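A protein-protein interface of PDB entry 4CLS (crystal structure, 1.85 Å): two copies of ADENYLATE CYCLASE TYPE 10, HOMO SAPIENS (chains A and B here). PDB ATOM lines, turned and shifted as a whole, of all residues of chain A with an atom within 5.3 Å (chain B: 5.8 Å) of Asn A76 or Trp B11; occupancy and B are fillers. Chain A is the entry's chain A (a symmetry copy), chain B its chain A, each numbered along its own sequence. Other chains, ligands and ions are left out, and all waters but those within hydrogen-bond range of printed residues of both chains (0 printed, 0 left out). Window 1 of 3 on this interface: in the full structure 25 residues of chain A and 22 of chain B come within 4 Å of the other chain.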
ATOM      1  N   LEU A  71     -13.630 -19.401  23.554  1.00  0.00           N
ATOM      2  CA  LEU A  71     -15.071 -19.268  23.562  1.00  0.00           C
ATOM      3  C   LEU A  71     -15.490 -17.912  22.998  1.00  0.00           C
ATOM      4  O   LEU A  71     -16.392 -17.834  22.116  1.00  0.00           O
ATOM      5  CB  LEU A  71     -15.622 -19.479  24.959  1.00  0.00           C
ATOM      6  CG  LEU A  71     -17.136 -19.268  25.085  1.00  0.00           C
ATOM      7  CD1 LEU A  71     -17.875 -20.437  24.438  1.00  0.00           C
ATOM      8  CD2 LEU A  71     -17.518 -19.093  26.536  1.00  0.00           C
ATOM      9  N   VAL A  72     -14.858 -16.871  23.470  1.00  0.00           N
ATOM     10  CA  VAL A  72     -15.208 -15.534  23.003  1.00  0.00           C
ATOM     11  C   VAL A  72     -14.908 -15.360  21.540  1.00  0.00           C
ATOM     12  O   VAL A  72     -15.677 -14.721  20.848  1.00  0.00           O
ATOM     13  CB  VAL A  72     -14.642 -14.399  23.864  1.00  0.00           C
ATOM     14  CG1 VAL A  72     -13.213 -14.101  23.599  1.00  0.00           C
ATOM     15  CG2 VAL A  72     -15.449 -13.119  23.594  1.00  0.00           C
ATOM     16  N   GLU A  73     -13.856 -15.996  21.048  1.00  0.00           N
ATOM     17  CA  GLU A  73     -13.529 -15.943  19.607  1.00  0.00           C
ATOM     18  C   GLU A  73     -14.627 -16.585  18.743  1.00  0.00           C
ATOM     19  O   GLU A  73     -15.079 -15.979  17.764  1.00  0.00           O
ATOM     20  CB  GLU A  73     -12.178 -16.653  19.402  1.00  0.00           C
ATOM     21  CG  GLU A  73     -11.719 -16.633  17.959  1.00  0.00           C
ATOM     22  CD  GLU A  73     -10.380 -17.344  17.810  1.00  0.00           C
ATOM     23  OE1 GLU A  73      -9.977 -18.092  18.752  1.00  0.00           O
ATOM     24  OE2 GLU A  73      -9.815 -17.164  16.748  1.00  0.00           O
ATOM     25  N   ILE A  74     -15.007 -17.794  19.084  1.00  0.00           N
ATOM     26  CA  ILE A  74     -15.996 -18.535  18.298  1.00  0.00           C
ATOM     27  C   ILE A  74     -17.362 -17.883  18.466  1.00  0.00           C
ATOM     28  O   ILE A  74     -18.061 -17.711  17.474  1.00  0.00           O
ATOM     29  CB  ILE A  74     -15.988 -20.023  18.540  1.00  0.00           C
ATOM     30  CG1 ILE A  74     -16.738 -20.781  17.466  1.00  0.00           C
ATOM     31  CG2 ILE A  74     -16.555 -20.400  19.883  1.00  0.00           C
ATOM     32  CD1 ILE A  74     -16.280 -20.541  16.050  1.00  0.00           C
ATOM     33  N   LEU A  75     -17.704 -17.466  19.678  1.00  0.00           N
ATOM     34  CA  LEU A  75     -18.986 -16.758  19.859  1.00  0.00           C
ATOM     35  C   LEU A  75     -19.055 -15.462  19.049  1.00  0.00           C
ATOM     36  O   LEU A  75     -20.014 -15.209  18.264  1.00  0.00           O
ATOM     37  CB  LEU A  75     -19.189 -16.453  21.307  1.00  0.00           C
ATOM     38  CG  LEU A  75     -20.498 -15.727  21.565  1.00  0.00           C
ATOM     39  CD1 LEU A  75     -21.726 -16.554  21.199  1.00  0.00           C
ATOM     40  CD2 LEU A  75     -20.532 -15.428  23.021  1.00  0.00           C
ATOM     41  N   ASN A  76     -18.036 -14.640  19.178  1.00  0.00           N
ATOM     42  CA  ASN A  76     -18.041 -13.391  18.443  1.00  0.00           C
ATOM     43  C   ASN A  76     -17.981 -13.520  16.943  1.00  0.00           C
ATOM     44  O   ASN A  76     -18.553 -12.690  16.200  1.00  0.00           O
ATOM     45  CB  ASN A  76     -16.980 -12.410  18.934  1.00  0.00           C
ATOM     46  CG  ASN A  76     -17.380 -11.750  20.240  1.00  0.00           C
ATOM     47  OD1 ASN A  76     -18.524 -11.871  20.661  1.00  0.00           O
ATOM     48  ND2 ASN A  76     -16.451 -11.148  20.898  1.00  0.00           N
ATOM     49  N   TYR A  77     -17.384 -14.577  16.493  1.00  0.00           N
ATOM     50  CA  TYR A  77     -17.314 -14.817  15.037  1.00  0.00           C
ATOM     51  C   TYR A  77     -18.766 -15.001  14.504  1.00  0.00           C
ATOM     52  O   TYR A  77     -19.173 -14.409  13.483  1.00  0.00           O
ATOM     53  CB  TYR A  77     -16.440 -16.018  14.755  1.00  0.00           C
ATOM     54  CG  TYR A  77     -16.453 -16.464  13.285  1.00  0.00           C
ATOM     55  CD1 TYR A  77     -16.038 -15.611  12.266  1.00  0.00           C
ATOM     56  CD2 TYR A  77     -16.883 -17.710  12.951  1.00  0.00           C
ATOM     57  CE1 TYR A  77     -16.025 -16.033  10.924  1.00  0.00           C
ATOM     58  CE2 TYR A  77     -16.881 -18.137  11.621  1.00  0.00           C
ATOM     59  CZ  TYR A  77     -16.484 -17.275  10.630  1.00  0.00           C
ATOM     60  OH  TYR A  77     -16.531 -17.727   9.347  1.00  0.00           O
ATOM     61  N   HIS A  78     -19.525 -15.793  15.221  1.00  0.00           N
ATOM     62  CA  HIS A  78     -20.902 -16.054  14.837  1.00  0.00           C
ATOM     63  C   HIS A  78     -21.825 -14.885  15.160  1.00  0.00           C
ATOM     64  O   HIS A  78     -22.560 -14.497  14.301  1.00  0.00           O
ATOM     65  CB  HIS A  78     -21.392 -17.302  15.507  1.00  0.00           C
ATOM     66  CG  HIS A  78     -20.750 -18.534  14.991  1.00  0.00           C
ATOM     67  ND1 HIS A  78     -20.702 -18.845  13.647  1.00  0.00           N
ATOM     68  CD2 HIS A  78     -20.020 -19.471  15.612  1.00  0.00           C
ATOM     69  CE1 HIS A  78     -20.026 -19.968  13.486  1.00  0.00           C
ATOM     70  NE2 HIS A  78     -19.626 -20.372  14.665  1.00  0.00           N
ATOM     71  N   ILE A  79     -21.727 -14.293  16.352  1.00  0.00           N
ATOM     72  CA  ILE A  79     -22.576 -13.191  16.706  1.00  0.00           C
ATOM     73  C   ILE A  79     -22.329 -11.980  15.834  1.00  0.00           C
ATOM     74  O   ILE A  79     -23.306 -11.313  15.397  1.00  0.00           O
ATOM     75  CB  ILE A  79     -22.462 -12.862  18.187  1.00  0.00           C
ATOM     76  CG1 ILE A  79     -23.106 -14.022  18.922  1.00  0.00           C
ATOM     77  CG2 ILE A  79     -23.195 -11.572  18.515  1.00  0.00           C
ATOM     78  CD1 ILE A  79     -23.086 -13.850  20.409  1.00  0.00           C
ATOM     79  N   SER A  80     -21.059 -11.726  15.494  1.00  0.00           N
ATOM     80  CA  SER A  80     -20.732 -10.629  14.604  1.00  0.00           C
ATOM     81  C   SER A  80     -21.469 -10.665  13.277  1.00  0.00           C
ATOM     82  O   SER A  80     -21.851  -9.621  12.776  1.00  0.00           O
ATOM     83  CB  SER A  80     -19.221 -10.619  14.230  1.00  0.00           C
ATOM     84  OG  SER A  80     -18.655 -10.007  15.302  1.00  0.00           O
ATOM     85  N   ALA A  81     -21.638 -11.838  12.715  1.00  0.00           N
ATOM     86  CA  ALA A  81     -22.304 -11.979  11.484  1.00  0.00           C
ATOM     87  C   ALA A  81     -23.796 -11.633  11.570  1.00  0.00           C
ATOM     88  O   ALA A  81     -24.344 -11.069  10.604  1.00  0.00           O
ATOM     89  CB  ALA A  81     -22.139 -13.414  10.919  1.00  0.00           C
ATOM     90  N   ILE A 395     -16.668  -9.404  26.571  1.00  0.00           N
ATOM     91  CA  ILE A 395     -17.313  -8.507  25.614  1.00  0.00           C
ATOM     92  C   ILE A 395     -17.752  -9.310  24.391  1.00  0.00           C
ATOM     93  O   ILE A 395     -16.947  -9.876  23.626  1.00  0.00           O
ATOM     94  CB  ILE A 395     -16.417  -7.320  25.231  1.00  0.00           C
ATOM     95  CG1 ILE A 395     -16.201  -6.446  26.484  1.00  0.00           C
ATOM     96  CG2 ILE A 395     -17.106  -6.502  24.158  1.00  0.00           C
ATOM     97  CD1 ILE A 395     -15.107  -5.437  26.328  1.00  0.00           C
ATOM     98  N   VAL A 396     -19.053  -9.348  24.206  1.00  0.00           N
ATOM     99  CA  VAL A 396     -19.659 -10.122  23.146  1.00  0.00           C
ATOM    100  C   VAL A 396     -20.312  -9.238  22.087  1.00  0.00           C
ATOM    101  O   VAL A 396     -20.954  -8.265  22.406  1.00  0.00           O
ATOM    102  CB  VAL A 396     -20.703 -11.006  23.759  1.00  0.00           C
ATOM    103  CG1 VAL A 396     -21.545 -11.734  22.681  1.00  0.00           C
ATOM    104  CG2 VAL A 396     -20.036 -12.076  24.632  1.00  0.00           C
ATOM    105  N   GLY A 397     -20.122  -9.588  20.826  1.00  0.00           N
ATOM    106  CA  GLY A 397     -20.669  -8.815  19.740  1.00  0.00           C
ATOM    107  C   GLY A 397     -19.656  -8.518  18.678  1.00  0.00           C
ATOM    108  O   GLY A 397     -18.709  -9.265  18.465  1.00  0.00           O
ATOM    109  N   GLN B   9     -10.000  -9.330   9.884  1.00  0.00           N
ATOM    110  CA  GLN B   9     -10.134  -9.765  11.230  1.00  0.00           C
ATOM    111  C   GLN B   9      -8.898 -10.603  11.643  1.00  0.00           C
ATOM    112  O   GLN B   9      -8.345 -11.484  10.962  1.00  0.00           O
ATOM    113  CB  GLN B   9     -11.552 -10.277  11.610  1.00  0.00           C
ATOM    114  CG  GLN B   9     -11.893 -10.397  13.113  1.00  0.00           C
ATOM    115  CD  GLN B   9     -11.459  -9.261  14.013  1.00  0.00           C
ATOM    116  OE1 GLN B   9     -11.547  -8.100  13.645  1.00  0.00           O
ATOM    117  NE2 GLN B   9     -10.995  -9.605  15.229  1.00  0.00           N
ATOM    118  N   ASP B  10      -8.459 -10.154  12.782  1.00  0.00           N
ATOM    119  CA  ASP B  10      -7.208 -10.494  13.358  1.00  0.00           C
ATOM    120  C   ASP B  10      -7.562 -11.372  14.565  1.00  0.00           C
ATOM    121  O   ASP B  10      -7.021 -11.200  15.710  1.00  0.00           O
ATOM    122  CB  ASP B  10      -6.611  -9.143  13.636  1.00  0.00           C
ATOM    123  CG  ASP B  10      -5.419  -9.179  14.446  1.00  0.00           C
ATOM    124  OD1 ASP B  10      -4.411  -9.831  14.122  1.00  0.00           O
ATOM    125  OD2 ASP B  10      -5.544  -8.412  15.394  1.00  0.00           O
ATOM    126  N   TRP B  11      -8.340 -12.412  14.264  1.00  0.00           N
ATOM    127  CA  TRP B  11      -8.728 -13.417  15.284  1.00  0.00           C
ATOM    128  C   TRP B  11      -7.475 -14.079  15.871  1.00  0.00           C
ATOM    129  O   TRP B  11      -6.472 -14.191  15.150  1.00  0.00           O
ATOM    130  CB  TRP B  11      -9.532 -14.492  14.587  1.00  0.00           C
ATOM    131  CG  TRP B  11     -10.831 -14.029  13.951  1.00  0.00           C
ATOM    132  CD1 TRP B  11     -11.111 -13.953  12.618  1.00  0.00           C
ATOM    133  CD2 TRP B  11     -11.986 -13.565  14.634  1.00  0.00           C
ATOM    134  NE1 TRP B  11     -12.399 -13.487  12.452  1.00  0.00           N
ATOM    135  CE2 TRP B  11     -12.946 -13.238  13.675  1.00  0.00           C
ATOM    136  CE3 TRP B  11     -12.286 -13.378  15.960  1.00  0.00           C
ATOM    137  CZ2 TRP B  11     -14.213 -12.744  14.006  1.00  0.00           C
ATOM    138  CZ3 TRP B  11     -13.561 -12.903  16.308  1.00  0.00           C
ATOM    139  CH2 TRP B  11     -14.502 -12.582  15.337  1.00  0.00           C
ATOM    140  N   PRO B  12      -7.555 -14.611  17.094  1.00  0.00           N
ATOM    141  CA  PRO B  12      -6.497 -15.345  17.653  1.00  0.00           C
ATOM    142  C   PRO B  12      -6.008 -16.514  16.789  1.00  0.00           C
ATOM    143  O   PRO B  12      -4.810 -16.701  16.664  1.00  0.00           O
ATOM    144  CB  PRO B  12      -7.095 -15.866  18.948  1.00  0.00           C
ATOM    145  CG  PRO B  12      -8.034 -14.808  19.391  1.00  0.00           C
ATOM    146  CD  PRO B  12      -8.646 -14.392  18.097  1.00  0.00           C
ATOM    147  N   ILE B  13      -6.891 -17.237  16.095  1.00  0.00           N
ATOM    148  CA  ILE B  13      -6.389 -18.305  15.189  1.00  0.00           C
ATOM    149  C   ILE B  13      -5.451 -17.761  14.105  1.00  0.00           C
ATOM    150  O   ILE B  13      -4.491 -18.430  13.769  1.00  0.00           O
ATOM    151  CB  ILE B  13      -7.542 -19.190  14.620  1.00  0.00           C
ATOM    152  CG1 ILE B  13      -7.040 -20.537  14.106  1.00  0.00           C
ATOM    153  CG2 ILE B  13      -8.420 -18.458  13.642  1.00  0.00           C
ATOM    154  CD1 ILE B  13      -8.216 -21.461  13.744  1.00  0.00           C
ATOM    155  N   VAL B  14      -5.753 -16.595  13.573  1.00  0.00           N
ATOM    156  CA  VAL B  14      -4.915 -15.984  12.551  1.00  0.00           C
ATOM    157  C   VAL B  14      -3.556 -15.568  13.142  1.00  0.00           C
ATOM    158  O   VAL B  14      -2.503 -15.790  12.575  1.00  0.00           O
ATOM    159  CB  VAL B  14      -5.628 -14.778  11.933  1.00  0.00           C
ATOM    160  CG1 VAL B  14      -4.703 -14.003  11.020  1.00  0.00           C
ATOM    161  CG2 VAL B  14      -6.889 -15.209  11.185  1.00  0.00           C
ATOM    162  N   ARG B  15      -3.596 -14.983  14.311  1.00  0.00           N
ATOM    163  CA  ARG B  15      -2.384 -14.632  15.009  1.00  0.00           C
ATOM    164  C   ARG B  15      -1.498 -15.848  15.316  1.00  0.00           C
ATOM    165  O   ARG B  15      -0.264 -15.793  15.144  1.00  0.00           O
ATOM    166  CB  ARG B  15      -2.692 -13.836  16.268  1.00  0.00           C
ATOM    167  CG  ARG B  15      -3.386 -12.513  16.053  1.00  0.00           C
ATOM    168  CD  ARG B  15      -3.607 -11.852  17.430  1.00  0.00           C
ATOM    169  NE  ARG B  15      -3.936 -10.448  17.255  1.00  0.00           N
ATOM    170  CZ  ARG B  15      -3.976  -9.538  18.233  1.00  0.00           C
ATOM    171  NH1 ARG B  15      -3.708  -9.886  19.487  1.00  0.00           N
ATOM    172  NH2 ARG B  15      -4.209  -8.263  17.910  1.00  0.00           N
ATOM    173  N   ILE B  16      -2.098 -16.940  15.722  1.00  0.00           N
ATOM    174  CA  ILE B  16      -1.375 -18.176  15.970  1.00  0.00           C
ATOM    175  C   ILE B  16      -0.754 -18.676  14.663  1.00  0.00           C
ATOM    176  O   ILE B  16       0.409 -19.038  14.615  1.00  0.00           O
ATOM    177  CB  ILE B  16      -2.289 -19.210  16.649  1.00  0.00           C
ATOM    178  CG1 ILE B  16      -2.623 -18.769  18.086  1.00  0.00           C
ATOM    179  CG2 ILE B  16      -1.589 -20.567  16.691  1.00  0.00           C
ATOM    180  CD1 ILE B  16      -3.770 -19.524  18.709  1.00  0.00           C
ATOM    181  N   LEU B 255      -7.868 -17.381   7.636  1.00  0.00           N
ATOM    182  CA  LEU B 255      -8.359 -18.448   8.511  1.00  0.00           C
ATOM    183  C   LEU B 255      -9.448 -17.937   9.417  1.00  0.00           C
ATOM    184  O   LEU B 255      -9.357 -16.838   9.919  1.00  0.00           O
ATOM    185  CB  LEU B 255      -7.279 -18.985   9.413  1.00  0.00           C
ATOM    186  CG  LEU B 255      -6.290 -20.040   9.059  1.00  0.00           C
ATOM    187  CD1 LEU B 255      -5.477 -20.399  10.323  1.00  0.00           C
ATOM    188  CD2 LEU B 255      -7.004 -21.283   8.588  1.00  0.00           C
ATOM    189  N   LYS B 256     -10.470 -18.739   9.632  1.00  0.00           N
ATOM    190  CA  LYS B 256     -11.597 -18.343  10.462  1.00  0.00           C
ATOM    191  C   LYS B 256     -11.576 -19.174  11.738  1.00  0.00           C
ATOM    192  O   LYS B 256     -11.071 -20.275  11.749  1.00  0.00           O
ATOM    193  CB  LYS B 256     -12.929 -18.529   9.723  1.00  0.00           C
ATOM    194  CG  LYS B 256     -13.027 -17.604   8.488  1.00  0.00           C
ATOM    195  CD  LYS B 256     -12.761 -16.115   8.750  1.00  0.00           C
ATOM    196  CE  LYS B 256     -12.536 -15.418   7.404  1.00  0.00           C
ATOM    197  NZ  LYS B 256     -12.197 -14.004   7.522  1.00  0.00           N
ATOM    198  N   PRO B 257     -12.130 -18.647  12.823  1.00  0.00           N
ATOM    199  CA  PRO B 257     -12.217 -19.386  14.065  1.00  0.00           C
ATOM    200  C   PRO B 257     -12.721 -20.793  13.869  1.00  0.00           C
ATOM    201  O   PRO B 257     -13.723 -21.031  13.149  1.00  0.00           O
ATOM    202  CB  PRO B 257     -13.206 -18.554  14.881  1.00  0.00           C
ATOM    203  CG  PRO B 257     -12.778 -17.160  14.462  1.00  0.00           C
ATOM    204  CD  PRO B 257     -12.666 -17.291  12.990  1.00  0.00           C
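The backbone NH (N) of Ile B13 lies within hydrogen-bond range of the side-chain carboxylate (OE2) of Glu A73. The backbone nitrogen of Pro B12 sits close to the side-chain carboxylate of Glu A73.
The backbone NH of Gly A397 sits at hydrogen-bond distance from the side-chain amide oxygen of Asn A76, at 2.8 Å. O of Asn A76 is in hydrogen-bond range of OG of Ser A80. ND2 of Asn A76 sits at hydrogen-bond distance from O of Ile A395, 3.1 Å away.
Among the printed residues, merely in contact across the chains: Glu A73 with Trp B11 (3.4 Å), Glu A73 with Pro B257 (3.7 Å), Ile A74 with Pro B257 (3.8 Å), Asn A76 with Trp B11 (3.9 Å), Tyr A77 with Trp B11 (3.6 Å), Tyr A77 with Lys B256 (3.6 Å) and Tyr A77 with Pro B257 (3.8 Å).
Printed residues of chain B within 4 Å of Glu A73: Trp B11, Pro B12, Ile B13 and Pro B257. Of chain B, only Trp B11 comes within 4 Å of Asn A76. Of the printed residues of chain B, Tyr A77 touches Trp B11, Lys B256 and Pro B257. Ile A79 touches none of the printed residues of chain B. Of chain A, only Glu A73 (3.4 Å), Asn A76 (3.9 Å) and Tyr A77 (3.6 Å) come within 4 Å of Trp B11. Printed residues of chain A within 4 Å of Pro B12: Glu A73. Of the printed residues of chain A, Ile B13 touches Glu A73 (3.0 Å). Printed residues of chain A within 4 Å of Lys B256: Tyr A77. The nearest printed residue of chain B that does not touch Asn A76 is Pro B257 (6.8 Å).
Of the 11 printed residues of chain B, 5 touch a printed residue of chain A. Printed residues of chain B that touch a printed residue of chain A: Trp B11, Pro B12, Ile B13, Lys B256 and Pro B257. Hydrophobic or aromatic side chains of chain B that line the printed part of chain A: Trp B11, Pro B12, Ile B13 and Pro B257. Among the printed residues, no Asp or Glu carboxylate lies within 4 Å of a Lys or Arg side-chain nitrogen of the other chain.
No position is printed for both chains. Of the 9 pairs that touch across the chains among the printed residues, none has its exchanged pair printed and touching as well.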
